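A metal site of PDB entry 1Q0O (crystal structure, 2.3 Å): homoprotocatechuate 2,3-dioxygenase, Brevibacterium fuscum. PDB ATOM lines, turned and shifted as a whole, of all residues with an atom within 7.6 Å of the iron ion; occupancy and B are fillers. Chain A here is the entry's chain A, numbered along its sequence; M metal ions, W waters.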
ATOM      1  N   ASP A 154      25.668  20.465  18.937  1.00  0.00           N
ATOM      2  CA  ASP A 154      24.463  21.236  19.215  1.00  0.00           C
ATOM      3  C   ASP A 154      24.570  22.706  19.595  1.00  0.00           C
ATOM      4  O   ASP A 154      23.773  23.523  19.149  1.00  0.00           O
ATOM      5  CB  ASP A 154      23.638  20.551  20.284  1.00  0.00           C
ATOM      6  CG  ASP A 154      22.354  21.286  20.579  1.00  0.00           C
ATOM      7  OD1 ASP A 154      21.351  21.061  19.891  1.00  0.00           O
ATOM      8  OD2 ASP A 154      22.361  22.127  21.491  1.00  0.00           O
ATOM      9  N   HIS A 155      25.517  23.063  20.441  1.00  0.00           N
ATOM     10  CA  HIS A 155      25.620  24.468  20.869  1.00  0.00           C
ATOM     11  C   HIS A 155      26.959  24.753  21.493  1.00  0.00           C
ATOM     12  O   HIS A 155      27.732  23.822  21.749  1.00  0.00           O
ATOM     13  CB  HIS A 155      24.532  24.825  21.915  1.00  0.00           C
ATOM     14  CG  HIS A 155      24.634  24.069  23.219  1.00  0.00           C
ATOM     15  ND1 HIS A 155      23.902  22.928  23.481  1.00  0.00           N
ATOM     16  CD2 HIS A 155      25.369  24.316  24.337  1.00  0.00           C
ATOM     17  CE1 HIS A 155      24.176  22.505  24.706  1.00  0.00           C
ATOM     18  NE2 HIS A 155      25.065  23.329  25.243  1.00  0.00           N
ATOM     19  N   PHE A 156      27.198  26.038  21.749  1.00  0.00           N
ATOM     20  CA  PHE A 156      28.413  26.495  22.421  1.00  0.00           C
ATOM     21  C   PHE A 156      27.839  27.224  23.619  1.00  0.00           C
ATOM     22  O   PHE A 156      26.636  27.511  23.667  1.00  0.00           O
ATOM     23  CB  PHE A 156      29.190  27.527  21.597  1.00  0.00           C
ATOM     24  CG  PHE A 156      29.615  27.054  20.224  1.00  0.00           C
ATOM     25  CD1 PHE A 156      30.399  25.923  20.069  1.00  0.00           C
ATOM     26  CD2 PHE A 156      29.320  27.800  19.095  1.00  0.00           C
ATOM     27  CE1 PHE A 156      30.879  25.534  18.795  1.00  0.00           C
ATOM     28  CE2 PHE A 156      29.794  27.430  17.811  1.00  0.00           C
ATOM     29  CZ  PHE A 156      30.577  26.291  17.662  1.00  0.00           C
ATOM     30  N   ASN A 157      28.683  27.493  24.602  1.00  0.00           N
ATOM     31  CA  ASN A 157      28.247  28.264  25.744  1.00  0.00           C
ATOM     32  C   ASN A 157      29.408  29.203  26.093  1.00  0.00           C
ATOM     33  O   ASN A 157      30.520  28.764  26.330  1.00  0.00           O
ATOM     34  CB  ASN A 157      27.897  27.364  26.915  1.00  0.00           C
ATOM     35  CG  ASN A 157      27.335  28.150  28.107  1.00  0.00           C
ATOM     36  OD1 ASN A 157      27.998  29.032  28.669  1.00  0.00           O
ATOM     37  ND2 ASN A 157      26.104  27.827  28.508  1.00  0.00           N
ATOM     38  N   TRP A 192      19.948  31.841  26.800  1.00  0.00           N
ATOM     39  CA  TRP A 192      20.082  30.843  25.752  1.00  0.00           C
ATOM     40  C   TRP A 192      19.461  31.425  24.485  1.00  0.00           C
ATOM     41  O   TRP A 192      18.356  31.941  24.516  1.00  0.00           O
ATOM     42  CB  TRP A 192      19.333  29.578  26.194  1.00  0.00           C
ATOM     43  CG  TRP A 192      20.046  28.714  27.226  1.00  0.00           C
ATOM     44  CD1 TRP A 192      20.710  27.553  26.973  1.00  0.00           C
ATOM     45  CD2 TRP A 192      20.172  28.957  28.640  1.00  0.00           C
ATOM     46  NE1 TRP A 192      21.252  27.065  28.126  1.00  0.00           N
ATOM     47  CE2 TRP A 192      20.929  27.893  29.175  1.00  0.00           C
ATOM     48  CE3 TRP A 192      19.713  29.963  29.520  1.00  0.00           C
ATOM     49  CZ2 TRP A 192      21.255  27.802  30.542  1.00  0.00           C
ATOM     50  CZ3 TRP A 192      20.035  29.868  30.880  1.00  0.00           C
ATOM     51  CH2 TRP A 192      20.799  28.795  31.375  1.00  0.00           C
ATOM     52  N   HIS A 200      19.124  26.179  21.741  1.00  0.00           N
ATOM     53  CA  HIS A 200      20.200  27.143  21.496  1.00  0.00           C
ATOM     54  C   HIS A 200      21.342  26.695  20.592  1.00  0.00           C
ATOM     55  O   HIS A 200      21.573  25.472  20.422  1.00  0.00           O
ATOM     56  CB  HIS A 200      20.794  27.650  22.826  1.00  0.00           C
ATOM     57  CG  HIS A 200      21.458  26.589  23.673  1.00  0.00           C
ATOM     58  ND1 HIS A 200      20.899  25.353  23.899  1.00  0.00           N
ATOM     59  CD2 HIS A 200      22.555  26.652  24.475  1.00  0.00           C
ATOM     60  CE1 HIS A 200      21.621  24.714  24.807  1.00  0.00           C
ATOM     61  NE2 HIS A 200      22.618  25.478  25.173  1.00  0.00           N
ATOM     62  N   ALA A 203      25.019  30.331  24.046  1.00  0.00           N
ATOM     63  CA  ALA A 203      24.423  30.809  25.286  1.00  0.00           C
ATOM     64  C   ALA A 203      25.406  31.658  26.035  1.00  0.00           C
ATOM     65  O   ALA A 203      26.612  31.534  25.898  1.00  0.00           O
ATOM     66  CB  ALA A 203      24.007  29.604  26.139  1.00  0.00           C
ATOM     67  N   THR A 205      26.850  32.778  29.693  1.00  0.00           N
ATOM     68  CA  THR A 205      26.890  32.473  31.110  1.00  0.00           C
ATOM     69  C   THR A 205      27.664  33.601  31.758  1.00  0.00           C
ATOM     70  O   THR A 205      28.794  33.870  31.361  1.00  0.00           O
ATOM     71  CB  THR A 205      27.567  31.143  31.337  1.00  0.00           C
ATOM     72  OG1 THR A 205      26.794  30.125  30.678  1.00  0.00           O
ATOM     73  CG2 THR A 205      27.668  30.850  32.831  1.00  0.00           C
ATOM     74  N   HIS A 213      32.787  28.285  27.910  1.00  0.00           N
ATOM     75  CA  HIS A 213      32.378  27.398  28.970  1.00  0.00           C
ATOM     76  C   HIS A 213      32.370  25.951  28.502  1.00  0.00           C
ATOM     77  O   HIS A 213      32.855  25.041  29.198  1.00  0.00           O
ATOM     78  CB  HIS A 213      31.001  27.806  29.498  1.00  0.00           C
ATOM     79  CG  HIS A 213      30.662  27.156  30.798  1.00  0.00           C
ATOM     80  ND1 HIS A 213      30.298  25.832  30.889  1.00  0.00           N
ATOM     81  CD2 HIS A 213      30.757  27.612  32.080  1.00  0.00           C
ATOM     82  CE1 HIS A 213      30.196  25.495  32.168  1.00  0.00           C
ATOM     83  NE2 HIS A 213      30.480  26.556  32.909  1.00  0.00           N
ATOM     84  N   HIS A 214      31.808  25.698  27.327  1.00  0.00           N
ATOM     85  CA  HIS A 214      31.760  24.339  26.779  1.00  0.00           C
ATOM     86  C   HIS A 214      31.227  24.281  25.353  1.00  0.00           C
ATOM     87  O   HIS A 214      30.680  25.253  24.826  1.00  0.00           O
ATOM     88  CB  HIS A 214      30.921  23.409  27.661  1.00  0.00           C
ATOM     89  CG  HIS A 214      29.475  23.798  27.768  1.00  0.00           C
ATOM     90  ND1 HIS A 214      28.979  24.542  28.814  1.00  0.00           N
ATOM     91  CD2 HIS A 214      28.406  23.444  27.005  1.00  0.00           C
ATOM     92  CE1 HIS A 214      27.651  24.626  28.698  1.00  0.00           C
ATOM     93  NE2 HIS A 214      27.285  23.977  27.605  1.00  0.00           N
ATOM     94  N   VAL A 215      31.428  23.115  24.738  1.00  0.00           N
ATOM     95  CA  VAL A 215      30.943  22.799  23.412  1.00  0.00           C
ATOM     96  C   VAL A 215      30.040  21.601  23.720  1.00  0.00           C
ATOM     97  O   VAL A 215      30.345  20.813  24.627  1.00  0.00           O
ATOM     98  CB  VAL A 215      32.098  22.362  22.493  1.00  0.00           C
ATOM     99  CG1 VAL A 215      31.562  21.767  21.231  1.00  0.00           C
ATOM    100  CG2 VAL A 215      32.959  23.550  22.176  1.00  0.00           C
ATOM    101  N   ALA A 216      28.944  21.437  23.003  1.00  0.00           N
ATOM    102  CA  ALA A 216      28.057  20.330  23.345  1.00  0.00           C
ATOM    103  C   ALA A 216      27.685  19.472  22.159  1.00  0.00           C
ATOM    104  O   ALA A 216      27.458  19.995  21.066  1.00  0.00           O
ATOM    105  CB  ALA A 216      26.794  20.862  24.003  1.00  0.00           C
ATOM    106  N   HIS A 248      18.308  18.886  32.799  1.00  0.00           N
ATOM    107  CA  HIS A 248      18.398  20.323  33.009  1.00  0.00           C
ATOM    108  C   HIS A 248      16.997  20.843  33.268  1.00  0.00           C
ATOM    109  O   HIS A 248      16.043  20.231  32.810  1.00  0.00           O
ATOM    110  CB  HIS A 248      18.862  21.029  31.745  1.00  0.00           C
ATOM    111  CG  HIS A 248      20.325  21.016  31.539  1.00  0.00           C
ATOM    112  ND1 HIS A 248      21.220  21.385  32.544  1.00  0.00           N
ATOM    113  CD2 HIS A 248      21.072  20.729  30.456  1.00  0.00           C
ATOM    114  CE1 HIS A 248      22.449  21.324  32.063  1.00  0.00           C
ATOM    115  NE2 HIS A 248      22.387  20.930  30.800  1.00  0.00           N
ATOM    116  N   SER A 251      16.031  24.391  29.344  1.00  0.00           N
ATOM    117  CA  SER A 251      16.251  23.595  28.116  1.00  0.00           C
ATOM    118  C   SER A 251      15.698  22.174  28.170  1.00  0.00           C
ATOM    119  O   SER A 251      15.616  21.511  27.150  1.00  0.00           O
ATOM    120  CB  SER A 251      17.731  23.543  27.711  1.00  0.00           C
ATOM    121  OG  SER A 251      18.345  22.357  28.173  1.00  0.00           O
ATOM    122  N   TYR A 255      21.565  15.733  30.391  1.00  0.00           N
ATOM    123  CA  TYR A 255      22.948  16.176  30.142  1.00  0.00           C
ATOM    124  C   TYR A 255      24.047  15.528  30.915  1.00  0.00           C
ATOM    125  O   TYR A 255      23.811  14.796  31.859  1.00  0.00           O
ATOM    126  CB  TYR A 255      23.096  17.670  30.386  1.00  0.00           C
ATOM    127  CG  TYR A 255      23.026  17.977  31.843  1.00  0.00           C
ATOM    128  CD1 TYR A 255      21.799  18.062  32.496  1.00  0.00           C
ATOM    129  CD2 TYR A 255      24.175  18.082  32.598  1.00  0.00           C
ATOM    130  CE1 TYR A 255      21.726  18.237  33.872  1.00  0.00           C
ATOM    131  CE2 TYR A 255      24.118  18.256  33.992  1.00  0.00           C
ATOM    132  CZ  TYR A 255      22.888  18.329  34.615  1.00  0.00           C
ATOM    133  OH  TYR A 255      22.845  18.521  35.988  1.00  0.00           O
ATOM    134  N   TYR A 257      28.486  16.637  31.732  1.00  0.00           N
ATOM    135  CA  TYR A 257      29.637  17.489  31.453  1.00  0.00           C
ATOM    136  C   TYR A 257      30.870  16.695  31.802  1.00  0.00           C
ATOM    137  O   TYR A 257      30.943  16.121  32.872  1.00  0.00           O
ATOM    138  CB  TYR A 257      29.633  18.770  32.305  1.00  0.00           C
ATOM    139  CG  TYR A 257      28.482  19.704  31.987  1.00  0.00           C
ATOM    140  CD1 TYR A 257      28.539  20.594  30.916  1.00  0.00           C
ATOM    141  CD2 TYR A 257      27.327  19.690  32.777  1.00  0.00           C
ATOM    142  CE1 TYR A 257      27.483  21.456  30.646  1.00  0.00           C
ATOM    143  CE2 TYR A 257      26.277  20.533  32.517  1.00  0.00           C
ATOM    144  CZ  TYR A 257      26.352  21.419  31.479  1.00  0.00           C
ATOM    145  OH  TYR A 257      25.297  22.300  31.344  1.00  0.00           O
ATOM    146  N   GLU A 267      29.957  18.989  26.706  1.00  0.00           N
ATOM    147  CA  GLU A 267      28.656  18.586  27.231  1.00  0.00           C
ATOM    148  C   GLU A 267      27.980  17.609  26.282  1.00  0.00           C
ATOM    149  O   GLU A 267      27.968  17.853  25.069  1.00  0.00           O
ATOM    150  CB  GLU A 267      27.728  19.802  27.466  1.00  0.00           C
ATOM    151  CG  GLU A 267      26.301  19.397  27.782  1.00  0.00           C
ATOM    152  CD  GLU A 267      25.358  20.586  28.044  1.00  0.00           C
ATOM    153  OE1 GLU A 267      25.574  21.703  27.507  1.00  0.00           O
ATOM    154  OE2 GLU A 267      24.365  20.437  28.778  1.00  0.00           O
ATOM    155  N   ILE A 268      27.479  16.494  26.810  1.00  0.00           N
ATOM    156  CA  ILE A 268      26.709  15.549  26.002  1.00  0.00           C
ATOM    157  C   ILE A 268      25.261  15.811  26.430  1.00  0.00           C
ATOM    158  O   ILE A 268      24.882  15.778  27.604  1.00  0.00           O
ATOM    159  CB  ILE A 268      27.100  14.091  26.176  1.00  0.00           C
ATOM    160  CG1 ILE A 268      28.507  13.852  25.606  1.00  0.00           C
ATOM    161  CG2 ILE A 268      26.190  13.266  25.285  1.00  0.00           C
ATOM    162  CD1 ILE A 268      29.617  14.379  26.398  1.00  0.00           C
ATOM    163  N   TYR A 269      24.437  16.065  25.446  1.00  0.00           N
ATOM    164  CA  TYR A 269      23.109  16.583  25.690  1.00  0.00           C
ATOM    165  C   TYR A 269      22.081  15.914  24.813  1.00  0.00           C
ATOM    166  O   TYR A 269      22.423  15.425  23.732  1.00  0.00           O
ATOM    167  CB  TYR A 269      23.307  18.068  25.353  1.00  0.00           C
ATOM    168  CG  TYR A 269      22.156  18.987  25.222  1.00  0.00           C
ATOM    169  CD1 TYR A 269      21.354  18.985  24.079  1.00  0.00           C
ATOM    170  CD2 TYR A 269      21.954  19.983  26.188  1.00  0.00           C
ATOM    171  CE1 TYR A 269      20.386  19.986  23.904  1.00  0.00           C
ATOM    172  CE2 TYR A 269      20.996  20.970  26.030  1.00  0.00           C
ATOM    173  CZ  TYR A 269      20.218  20.973  24.884  1.00  0.00           C
ATOM    174  OH  TYR A 269      19.309  22.006  24.746  1.00  0.00           O
ATOM    175  N   ARG A 293      18.802  24.518  37.122  1.00  0.00           N
ATOM    176  CA  ARG A 293      19.968  23.955  36.449  1.00  0.00           C
ATOM    177  C   ARG A 293      19.830  22.446  36.347  1.00  0.00           C
ATOM    178  O   ARG A 293      19.949  21.874  35.251  1.00  0.00           O
ATOM    179  CB  ARG A 293      21.254  24.307  37.220  1.00  0.00           C
ATOM    180  CG  ARG A 293      21.644  25.765  37.169  1.00  0.00           C
ATOM    181  CD  ARG A 293      22.588  26.015  36.052  1.00  0.00           C
ATOM    182  NE  ARG A 293      22.925  27.425  35.929  1.00  0.00           N
ATOM    183  CZ  ARG A 293      23.285  27.982  34.777  1.00  0.00           C
ATOM    184  NH1 ARG A 293      23.358  27.238  33.668  1.00  0.00           N
ATOM    185  NH2 ARG A 293      23.564  29.274  34.719  1.00  0.00           N
ATOM    186  N   TRP A 304      32.115  24.232  37.966  1.00  0.00           N
ATOM    187  CA  TRP A 304      31.286  24.496  36.787  1.00  0.00           C
ATOM    188  C   TRP A 304      31.138  26.012  36.619  1.00  0.00           C
ATOM    189  O   TRP A 304      31.162  26.529  35.504  1.00  0.00           O
ATOM    190  CB  TRP A 304      29.918  23.856  36.963  1.00  0.00           C
ATOM    191  CG  TRP A 304      29.180  23.701  35.686  1.00  0.00           C
ATOM    192  CD1 TRP A 304      29.309  22.679  34.781  1.00  0.00           C
ATOM    193  CD2 TRP A 304      28.239  24.618  35.132  1.00  0.00           C
ATOM    194  NE1 TRP A 304      28.501  22.910  33.694  1.00  0.00           N
ATOM    195  CE2 TRP A 304      27.834  24.101  33.887  1.00  0.00           C
ATOM    196  CE3 TRP A 304      27.697  25.840  35.569  1.00  0.00           C
ATOM    197  CZ2 TRP A 304      26.916  24.764  33.051  1.00  0.00           C
ATOM    198  CZ3 TRP A 304      26.781  26.492  34.753  1.00  0.00           C
ATOM    199  CH2 TRP A 304      26.400  25.956  33.507  1.00  0.00           C
HETATM  200 FE    FE M   1      25.072  23.604  27.439  1.00  0.00          FE
HETATM  201  O   HOH W   1      22.517  23.534  28.037  1.00  0.00           O
HETATM  202  O   HOH W   2      24.786  25.438  27.237  1.00  0.00           O
HETATM  203  O   HOH W   3      24.039  24.669  30.074  1.00  0.00           O
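The iron ion is bound by water W2, the side-chain carboxylate of Glu 267, a ring nitrogen (NE2) of His 155 and a ring nitrogen (NE2) of His 214. The iron ion has four donor atoms within binding distance. Slightly farther from the iron ion lies water W1 (2.6 Å).
Water W2 bridges a ring nitrogen (NE2) of His 200 (3.0 Å) and the side-chain amide nitrogen of Asn 157 (3.0 Å).
His 200 touches the iron ion. Four residues have an atom within 4 Å of the iron ion: His 155, His 200, His 214 and Glu 267. The nearest printed residue that does not touch the iron ion is Tyr 257 (4.1 Å).
The side-chain carboxylate (OE2) of Glu 267 lies within hydrogen-bond range of the side-chain hydroxyl (OH) of Tyr 257 (3.3 Å). The side-chain carboxylate (OE2) of Glu 267 is in hydrogen-bond range of a ring nitrogen (NE2) of His 248 (2.9 Å). The backbone carbonyl oxygen of Val 215 sits at hydrogen-bond distance from the backbone NH of Glu 267 (2.8 Å). A ring nitrogen (NE2) of His 200 lies close to a ring nitrogen (ND1) of His 155 (3.3 Å). O of His 155 is in hydrogen-bond range of N of Ala 216 (3.0 Å). ND1 of His 155 sits at hydrogen-bond distance from OD2 of Asp 154 (2.6 Å). The backbone NH (N) of Asn 157 is in hydrogen-bond range of the backbone carbonyl oxygen (O) of His 214 (3.0 Å). A ring nitrogen (ND1) of His 214 sits at hydrogen-bond distance from a ring nitrogen (ND1) of His 213 (2.8 Å).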
